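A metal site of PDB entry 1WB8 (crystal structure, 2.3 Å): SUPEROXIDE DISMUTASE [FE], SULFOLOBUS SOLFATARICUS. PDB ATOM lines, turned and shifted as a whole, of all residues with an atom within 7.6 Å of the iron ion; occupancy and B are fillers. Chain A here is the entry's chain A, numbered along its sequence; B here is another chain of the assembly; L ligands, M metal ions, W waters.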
ATOM      1  N   HIS A  33     -26.969 -25.354 -22.744  1.00  0.00           N
ATOM      2  CA  HIS A  33     -26.625 -24.591 -23.940  1.00  0.00           C
ATOM      3  C   HIS A  33     -27.405 -25.083 -25.151  1.00  0.00           C
ATOM      4  O   HIS A  33     -27.872 -24.286 -25.968  1.00  0.00           O
ATOM      5  CB  HIS A  33     -25.118 -24.703 -24.210  1.00  0.00           C
ATOM      6  CG  HIS A  33     -24.572 -23.596 -25.057  1.00  0.00           C
ATOM      7  ND1 HIS A  33     -23.225 -23.423 -25.278  1.00  0.00           N
ATOM      8  CD2 HIS A  33     -25.192 -22.586 -25.723  1.00  0.00           C
ATOM      9  CE1 HIS A  33     -23.036 -22.347 -26.039  1.00  0.00           C
ATOM     10  NE2 HIS A  33     -24.218 -21.827 -26.323  1.00  0.00           N
ATOM     11  N   TYR A  34     -27.544 -26.405 -25.262  1.00  0.00           N
ATOM     12  CA  TYR A  34     -28.250 -27.023 -26.379  1.00  0.00           C
ATOM     13  C   TYR A  34     -29.754 -27.110 -26.123  1.00  0.00           C
ATOM     14  O   TYR A  34     -30.556 -26.646 -26.931  1.00  0.00           O
ATOM     15  CB  TYR A  34     -27.715 -28.427 -26.637  1.00  0.00           C
ATOM     16  CG  TYR A  34     -28.447 -29.186 -27.716  1.00  0.00           C
ATOM     17  CD1 TYR A  34     -28.355 -28.798 -29.050  1.00  0.00           C
ATOM     18  CD2 TYR A  34     -29.256 -30.278 -27.401  1.00  0.00           C
ATOM     19  CE1 TYR A  34     -29.046 -29.479 -30.060  1.00  0.00           C
ATOM     20  CE2 TYR A  34     -29.954 -30.962 -28.395  1.00  0.00           C
ATOM     21  CZ  TYR A  34     -29.842 -30.560 -29.711  1.00  0.00           C
ATOM     22  OH  TYR A  34     -30.545 -31.222 -30.698  1.00  0.00           O
ATOM     23  N   HIS A  37     -30.779 -22.786 -24.464  1.00  0.00           N
ATOM     24  CA  HIS A  37     -30.505 -21.684 -25.368  1.00  0.00           C
ATOM     25  C   HIS A  37     -30.795 -21.951 -26.845  1.00  0.00           C
ATOM     26  O   HIS A  37     -31.616 -21.266 -27.451  1.00  0.00           O
ATOM     27  CB  HIS A  37     -29.054 -21.233 -25.186  1.00  0.00           C
ATOM     28  CG  HIS A  37     -28.764 -20.700 -23.806  1.00  0.00           C
ATOM     29  ND1 HIS A  37     -29.278 -19.505 -23.350  1.00  0.00           N
ATOM     30  CD2 HIS A  37     -28.030 -21.215 -22.799  1.00  0.00           C
ATOM     31  CE1 HIS A  37     -28.871 -19.306 -22.104  1.00  0.00           C
ATOM     32  NE2 HIS A  37     -28.109 -20.331 -21.747  1.00  0.00           N
ATOM     33  N   HIS A  38     -30.139 -22.949 -27.439  1.00  0.00           N
ATOM     34  CA  HIS A  38     -30.353 -23.224 -28.856  1.00  0.00           C
ATOM     35  C   HIS A  38     -31.812 -23.566 -29.148  1.00  0.00           C
ATOM     36  O   HIS A  38     -32.389 -23.043 -30.088  1.00  0.00           O
ATOM     37  CB  HIS A  38     -29.440 -24.354 -29.342  1.00  0.00           C
ATOM     38  CG  HIS A  38     -29.433 -24.527 -30.834  1.00  0.00           C
ATOM     39  ND1 HIS A  38     -28.605 -25.423 -31.481  1.00  0.00           N
ATOM     40  CD2 HIS A  38     -30.164 -23.924 -31.802  1.00  0.00           C
ATOM     41  CE1 HIS A  38     -28.824 -25.361 -32.782  1.00  0.00           C
ATOM     42  NE2 HIS A  38     -29.768 -24.464 -33.005  1.00  0.00           N
ATOM     43  N   TYR A  41     -33.950 -20.461 -29.363  1.00  0.00           N
ATOM     44  CA  TYR A  41     -33.859 -19.653 -30.606  1.00  0.00           C
ATOM     45  C   TYR A  41     -34.677 -20.371 -31.680  1.00  0.00           C
ATOM     46  O   TYR A  41     -35.281 -19.577 -32.440  1.00  0.00           O
ATOM     47  CB  TYR A  41     -32.404 -19.432 -31.104  1.00  0.00           C
ATOM     48  CG  TYR A  41     -31.602 -18.608 -30.125  1.00  0.00           C
ATOM     49  CD1 TYR A  41     -32.042 -17.280 -29.807  1.00  0.00           C
ATOM     50  CD2 TYR A  41     -30.404 -19.124 -29.556  1.00  0.00           C
ATOM     51  CE1 TYR A  41     -31.304 -16.481 -28.939  1.00  0.00           C
ATOM     52  CE2 TYR A  41     -29.648 -18.298 -28.656  1.00  0.00           C
ATOM     53  CZ  TYR A  41     -30.124 -16.973 -28.368  1.00  0.00           C
ATOM     54  OH  TYR A  41     -29.357 -16.173 -27.511  1.00  0.00           O
ATOM     55  N   GLY A  80     -29.307 -16.774 -33.894  1.00  0.00           N
ATOM     56  CA  GLY A  80     -29.092 -17.522 -32.673  1.00  0.00           C
ATOM     57  C   GLY A  80     -29.117 -19.008 -33.018  1.00  0.00           C
ATOM     58  O   GLY A  80     -28.308 -19.791 -32.527  1.00  0.00           O
ATOM     59  N   LEU A  83     -26.089 -19.912 -35.948  1.00  0.00           N
ATOM     60  CA  LEU A  83     -24.745 -19.877 -35.374  1.00  0.00           C
ATOM     61  C   LEU A  83     -24.466 -21.017 -34.391  1.00  0.00           C
ATOM     62  O   LEU A  83     -23.348 -21.531 -34.348  1.00  0.00           O
ATOM     63  CB  LEU A  83     -24.481 -18.515 -34.704  1.00  0.00           C
ATOM     64  CG  LEU A  83     -24.444 -17.320 -35.660  1.00  0.00           C
ATOM     65  CD1 LEU A  83     -24.017 -16.066 -34.904  1.00  0.00           C
ATOM     66  CD2 LEU A  83     -23.475 -17.590 -36.821  1.00  0.00           C
ATOM     67  N   HIS A  84     -25.464 -21.416 -33.615  1.00  0.00           N
ATOM     68  CA  HIS A  84     -25.238 -22.512 -32.683  1.00  0.00           C
ATOM     69  C   HIS A  84     -25.106 -23.832 -33.432  1.00  0.00           C
ATOM     70  O   HIS A  84     -24.341 -24.694 -33.025  1.00  0.00           O
ATOM     71  CB  HIS A  84     -26.356 -22.594 -31.643  1.00  0.00           C
ATOM     72  CG  HIS A  84     -26.236 -21.579 -30.556  1.00  0.00           C
ATOM     73  ND1 HIS A  84     -26.733 -20.302 -30.664  1.00  0.00           N
ATOM     74  CD2 HIS A  84     -25.630 -21.646 -29.345  1.00  0.00           C
ATOM     75  CE1 HIS A  84     -26.441 -19.619 -29.577  1.00  0.00           C
ATOM     76  NE2 HIS A  84     -25.775 -20.410 -28.756  1.00  0.00           N
ATOM     77  N   TYR A  87     -21.701 -24.026 -34.538  1.00  0.00           N
ATOM     78  CA  TYR A  87     -20.851 -24.220 -33.353  1.00  0.00           C
ATOM     79  C   TYR A  87     -20.691 -25.693 -32.962  1.00  0.00           C
ATOM     80  O   TYR A  87     -19.581 -26.174 -32.782  1.00  0.00           O
ATOM     81  CB  TYR A  87     -21.456 -23.424 -32.193  1.00  0.00           C
ATOM     82  CG  TYR A  87     -20.686 -23.466 -30.902  1.00  0.00           C
ATOM     83  CD1 TYR A  87     -19.357 -23.027 -30.837  1.00  0.00           C
ATOM     84  CD2 TYR A  87     -21.293 -23.878 -29.722  1.00  0.00           C
ATOM     85  CE1 TYR A  87     -18.676 -22.984 -29.614  1.00  0.00           C
ATOM     86  CE2 TYR A  87     -20.634 -23.841 -28.509  1.00  0.00           C
ATOM     87  CZ  TYR A  87     -19.320 -23.392 -28.456  1.00  0.00           C
ATOM     88  OH  TYR A  87     -18.673 -23.351 -27.249  1.00  0.00           O
ATOM     89  N   TRP A  88     -21.810 -26.403 -32.813  1.00  0.00           N
ATOM     90  CA  TRP A  88     -21.766 -27.821 -32.448  1.00  0.00           C
ATOM     91  C   TRP A  88     -20.945 -28.644 -33.441  1.00  0.00           C
ATOM     92  O   TRP A  88     -20.121 -29.460 -33.045  1.00  0.00           O
ATOM     93  CB  TRP A  88     -23.191 -28.399 -32.386  1.00  0.00           C
ATOM     94  CG  TRP A  88     -24.143 -27.636 -31.520  1.00  0.00           C
ATOM     95  CD1 TRP A  88     -25.406 -27.258 -31.843  1.00  0.00           C
ATOM     96  CD2 TRP A  88     -23.904 -27.140 -30.195  1.00  0.00           C
ATOM     97  NE1 TRP A  88     -25.975 -26.554 -30.814  1.00  0.00           N
ATOM     98  CE2 TRP A  88     -25.078 -26.461 -29.785  1.00  0.00           C
ATOM     99  CE3 TRP A  88     -22.817 -27.197 -29.304  1.00  0.00           C
ATOM    100  CZ2 TRP A  88     -25.202 -25.849 -28.536  1.00  0.00           C
ATOM    101  CZ3 TRP A  88     -22.942 -26.586 -28.055  1.00  0.00           C
ATOM    102  CH2 TRP A  88     -24.132 -25.911 -27.686  1.00  0.00           C
ATOM    103  N   GLY A 134     -20.648 -12.168 -27.770  1.00  0.00           N
ATOM    104  CA  GLY A 134     -20.633 -12.302 -29.214  1.00  0.00           C
ATOM    105  C   GLY A 134     -19.949 -13.573 -29.673  1.00  0.00           C
ATOM    106  O   GLY A 134     -19.976 -14.587 -28.969  1.00  0.00           O
ATOM    107  N   TRP A 135     -19.331 -13.518 -30.848  1.00  0.00           N
ATOM    108  CA  TRP A 135     -18.643 -14.662 -31.435  1.00  0.00           C
ATOM    109  C   TRP A 135     -17.339 -14.248 -32.116  1.00  0.00           C
ATOM    110  O   TRP A 135     -17.147 -13.085 -32.466  1.00  0.00           O
ATOM    111  CB  TRP A 135     -19.517 -15.330 -32.509  1.00  0.00           C
ATOM    112  CG  TRP A 135     -20.892 -15.718 -32.075  1.00  0.00           C
ATOM    113  CD1 TRP A 135     -21.917 -14.878 -31.752  1.00  0.00           C
ATOM    114  CD2 TRP A 135     -21.390 -17.050 -31.892  1.00  0.00           C
ATOM    115  NE1 TRP A 135     -23.021 -15.614 -31.376  1.00  0.00           N
ATOM    116  CE2 TRP A 135     -22.727 -16.949 -31.448  1.00  0.00           C
ATOM    117  CE3 TRP A 135     -20.823 -18.328 -32.060  1.00  0.00           C
ATOM    118  CZ2 TRP A 135     -23.513 -18.071 -31.171  1.00  0.00           C
ATOM    119  CZ3 TRP A 135     -21.616 -19.459 -31.775  1.00  0.00           C
ATOM    120  CH2 TRP A 135     -22.945 -19.312 -31.333  1.00  0.00           C
ATOM    121  N   HIS A 155     -25.627 -11.797 -31.695  1.00  0.00           N
ATOM    122  CA  HIS A 155     -25.632 -12.823 -32.743  1.00  0.00           C
ATOM    123  C   HIS A 155     -25.736 -12.241 -34.154  1.00  0.00           C
ATOM    124  O   HIS A 155     -25.488 -12.936 -35.133  1.00  0.00           O
ATOM    125  CB  HIS A 155     -26.817 -13.789 -32.559  1.00  0.00           C
ATOM    126  CG  HIS A 155     -26.814 -14.525 -31.262  1.00  0.00           C
ATOM    127  ND1 HIS A 155     -25.896 -15.504 -30.960  1.00  0.00           N
ATOM    128  CD2 HIS A 155     -27.619 -14.427 -30.178  1.00  0.00           C
ATOM    129  CE1 HIS A 155     -26.124 -15.969 -29.752  1.00  0.00           C
ATOM    130  NE2 HIS A 155     -27.175 -15.335 -29.252  1.00  0.00           N
ATOM    131  N   ASP A 170     -18.248 -19.507 -29.813  1.00  0.00           N
ATOM    132  CA  ASP A 170     -19.296 -18.815 -29.073  1.00  0.00           C
ATOM    133  C   ASP A 170     -18.674 -18.081 -27.882  1.00  0.00           C
ATOM    134  O   ASP A 170     -18.035 -18.696 -27.042  1.00  0.00           O
ATOM    135  CB  ASP A 170     -20.332 -19.820 -28.575  1.00  0.00           C
ATOM    136  CG  ASP A 170     -21.551 -19.155 -27.957  1.00  0.00           C
ATOM    137  OD1 ASP A 170     -21.556 -17.920 -27.790  1.00  0.00           O
ATOM    138  OD2 ASP A 170     -22.505 -19.891 -27.633  1.00  0.00           O
ATOM    139  N   GLU A 171     -18.875 -16.770 -27.803  1.00  0.00           N
ATOM    140  CA  GLU A 171     -18.316 -16.018 -26.696  1.00  0.00           C
ATOM    141  C   GLU A 171     -19.359 -15.355 -25.798  1.00  0.00           C
ATOM    142  O   GLU A 171     -19.094 -14.317 -25.186  1.00  0.00           O
ATOM    143  CB  GLU A 171     -17.298 -14.982 -27.186  1.00  0.00           C
ATOM    144  CG  GLU A 171     -15.992 -15.585 -27.684  1.00  0.00           C
ATOM    145  CD  GLU A 171     -14.930 -14.537 -27.951  1.00  0.00           C
ATOM    146  OE1 GLU A 171     -14.392 -13.967 -26.978  1.00  0.00           O
ATOM    147  OE2 GLU A 171     -14.620 -14.300 -29.135  1.00  0.00           O
ATOM    148  N   PHE A 172     -20.550 -15.938 -25.729  1.00  0.00           N
ATOM    149  CA  PHE A 172     -21.575 -15.418 -24.842  1.00  0.00           C
ATOM    150  C   PHE A 172     -21.159 -16.027 -23.508  1.00  0.00           C
ATOM    151  O   PHE A 172     -20.572 -17.115 -23.479  1.00  0.00           O
ATOM    152  CB  PHE A 172     -22.959 -15.922 -25.219  1.00  0.00           C
ATOM    153  CG  PHE A 172     -23.770 -14.938 -25.996  1.00  0.00           C
ATOM    154  CD1 PHE A 172     -23.408 -14.588 -27.300  1.00  0.00           C
ATOM    155  CD2 PHE A 172     -24.907 -14.367 -25.430  1.00  0.00           C
ATOM    156  CE1 PHE A 172     -24.176 -13.688 -28.031  1.00  0.00           C
ATOM    157  CE2 PHE A 172     -25.685 -13.462 -26.153  1.00  0.00           C
ATOM    158  CZ  PHE A 172     -25.313 -13.117 -27.465  1.00  0.00           C
ATOM    159  N   GLU A 173     -21.467 -15.350 -22.419  1.00  0.00           N
ATOM    160  CA  GLU A 173     -21.088 -15.844 -21.105  1.00  0.00           C
ATOM    161  C   GLU A 173     -21.666 -17.222 -20.786  1.00  0.00           C
ATOM    162  O   GLU A 173     -21.042 -17.988 -20.052  1.00  0.00           O
ATOM    163  CB  GLU A 173     -21.490 -14.826 -20.043  1.00  0.00           C
ATOM    164  CG  GLU A 173     -20.826 -13.475 -20.267  1.00  0.00           C
ATOM    165  CD  GLU A 173     -21.337 -12.407 -19.325  1.00  0.00           C
ATOM    166  OE1 GLU A 173     -22.572 -12.237 -19.222  1.00  0.00           O
ATOM    167  OE2 GLU A 173     -20.513 -11.714 -18.695  1.00  0.00           O
ATOM    168  N   HIS A 174     -22.839 -17.539 -21.340  1.00  0.00           N
ATOM    169  CA  HIS A 174     -23.447 -18.837 -21.062  1.00  0.00           C
ATOM    170  C   HIS A 174     -22.644 -20.006 -21.638  1.00  0.00           C
ATOM    171  O   HIS A 174     -22.803 -21.138 -21.230  1.00  0.00           O
ATOM    172  CB  HIS A 174     -24.891 -18.901 -21.590  1.00  0.00           C
ATOM    173  CG  HIS A 174     -24.995 -18.834 -23.081  1.00  0.00           C
ATOM    174  ND1 HIS A 174     -25.558 -17.763 -23.744  1.00  0.00           N
ATOM    175  CD2 HIS A 174     -24.633 -19.724 -24.034  1.00  0.00           C
ATOM    176  CE1 HIS A 174     -25.534 -17.991 -25.050  1.00  0.00           C
ATOM    177  NE2 HIS A 174     -24.980 -19.176 -25.255  1.00  0.00           N
ATOM    178  N   ALA A 175     -21.750 -19.710 -22.579  1.00  0.00           N
ATOM    179  CA  ALA A 175     -20.960 -20.780 -23.185  1.00  0.00           C
ATOM    180  C   ALA A 175     -19.831 -21.260 -22.277  1.00  0.00           C
ATOM    181  O   ALA A 175     -19.243 -22.302 -22.536  1.00  0.00           O
ATOM    182  CB  ALA A 175     -20.384 -20.309 -24.513  1.00  0.00           C
ATOM    183  N   TYR A 187     -11.170 -20.112 -21.332  1.00  0.00           N
ATOM    184  CA  TYR A 187     -12.137 -20.845 -22.138  1.00  0.00           C
ATOM    185  C   TYR A 187     -11.672 -20.863 -23.587  1.00  0.00           C
ATOM    186  O   TYR A 187     -11.726 -21.898 -24.260  1.00  0.00           O
ATOM    187  CB  TYR A 187     -13.505 -20.176 -22.012  1.00  0.00           C
ATOM    188  CG  TYR A 187     -14.476 -20.474 -23.143  1.00  0.00           C
ATOM    189  CD1 TYR A 187     -14.977 -21.761 -23.335  1.00  0.00           C
ATOM    190  CD2 TYR A 187     -14.885 -19.469 -24.007  1.00  0.00           C
ATOM    191  CE1 TYR A 187     -15.879 -22.032 -24.385  1.00  0.00           C
ATOM    192  CE2 TYR A 187     -15.782 -19.716 -25.051  1.00  0.00           C
ATOM    193  CZ  TYR A 187     -16.278 -21.009 -25.222  1.00  0.00           C
ATOM    194  OH  TYR A 187     -17.160 -21.259 -26.247  1.00  0.00           O
ATOM    195  N   GLU B 173     -25.676 -12.041 -18.638  1.00  0.00           N
ATOM    196  CA  GLU B 173     -25.803 -13.370 -18.070  1.00  0.00           C
ATOM    197  C   GLU B 173     -25.010 -13.567 -16.791  1.00  0.00           C
ATOM    198  O   GLU B 173     -25.416 -14.353 -15.935  1.00  0.00           O
ATOM    199  CB  GLU B 173     -25.404 -14.411 -19.123  1.00  0.00           C
ATOM    200  CG  GLU B 173     -26.269 -14.309 -20.373  1.00  0.00           C
ATOM    201  CD  GLU B 173     -25.785 -15.207 -21.489  1.00  0.00           C
ATOM    202  OE1 GLU B 173     -24.582 -15.149 -21.825  1.00  0.00           O
ATOM    203  OE2 GLU B 173     -26.609 -15.959 -22.044  1.00  0.00           O
HETATM  204  C1  LIG L   1     -30.678 -16.816 -25.091  1.00  0.00           C
HETATM  205  S1  LIG L   1     -29.141 -16.473 -26.015  1.00  0.00           S
HETATM  206  C2  LIG L   1     -31.490 -15.588 -24.961  1.00  0.00           C
HETATM  207  C3  LIG L   1     -31.028 -14.471 -24.176  1.00  0.00           C
HETATM  208  C4  LIG L   1     -31.835 -13.271 -24.060  1.00  0.00           C
HETATM  209  C5  LIG L   1     -33.083 -13.211 -24.717  1.00  0.00           C
HETATM  210  C6  LIG L   1     -33.532 -14.338 -25.504  1.00  0.00           C
HETATM  211  C7  LIG L   1     -32.734 -15.504 -25.613  1.00  0.00           C
HETATM  212  O1  LIG L   1     -28.587 -15.195 -25.652  1.00  0.00           O
HETATM  213  O2  LIG L   1     -28.365 -17.684 -25.953  1.00  0.00           O
HETATM  214 FE    FE M   1     -24.388 -19.861 -27.170  1.00  0.00          FE
HETATM  215  O   HOH W   1     -24.345 -17.760 -27.899  1.00  0.00           O
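S1 of the ligand is bonded to OH of Tyr 41 (1.5 Å).
An oxygen (O2) of the ligand is in hydrogen-bond range of a ring nitrogen (ND1) of His 37.
The backbone carbonyl oxygen (O) of His 33 is in hydrogen-bond range of the backbone NH (N) of His 38 (3.0 Å).
The backbone NH (N) of Phe 172 sits at hydrogen-bond distance from the side-chain carboxylate (OD1) of Asp 170 (3.0 Å).
OH of Tyr 187 is in hydrogen-bond range of O of Asp 170 (2.8 Å).
A ring nitrogen (ND1) of His 174 lies within hydrogen-bond range of the side-chain carboxylate (OE2) of Glu 173 of chain B.
The backbone carbonyl oxygen (O) of His 84 lies close to the indole nitrogen (NE1) of Trp 88, 3.3 Å away.
O of Gly 80 sits at hydrogen-bond distance from ND1 of His 84.
Four residues have an atom within 4 Å of the iron ion: His 33, His 84, Asp 170 and His 174.
The nearest printed residue that does not touch the iron ion is Trp 135 (4.4 Å).
OD2 of Asp 170 binds the iron ion (1.9 Å).
A ring nitrogen (NE2) of His 174 is bound to the iron ion, at 2.1 Å.
A ring nitrogen (NE2) of His 33 is bound to the iron ion.
NE2 of His 84 is bound to the iron ion (2.2 Å).
The iron ion is bound by water W1 (2.2 Å).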
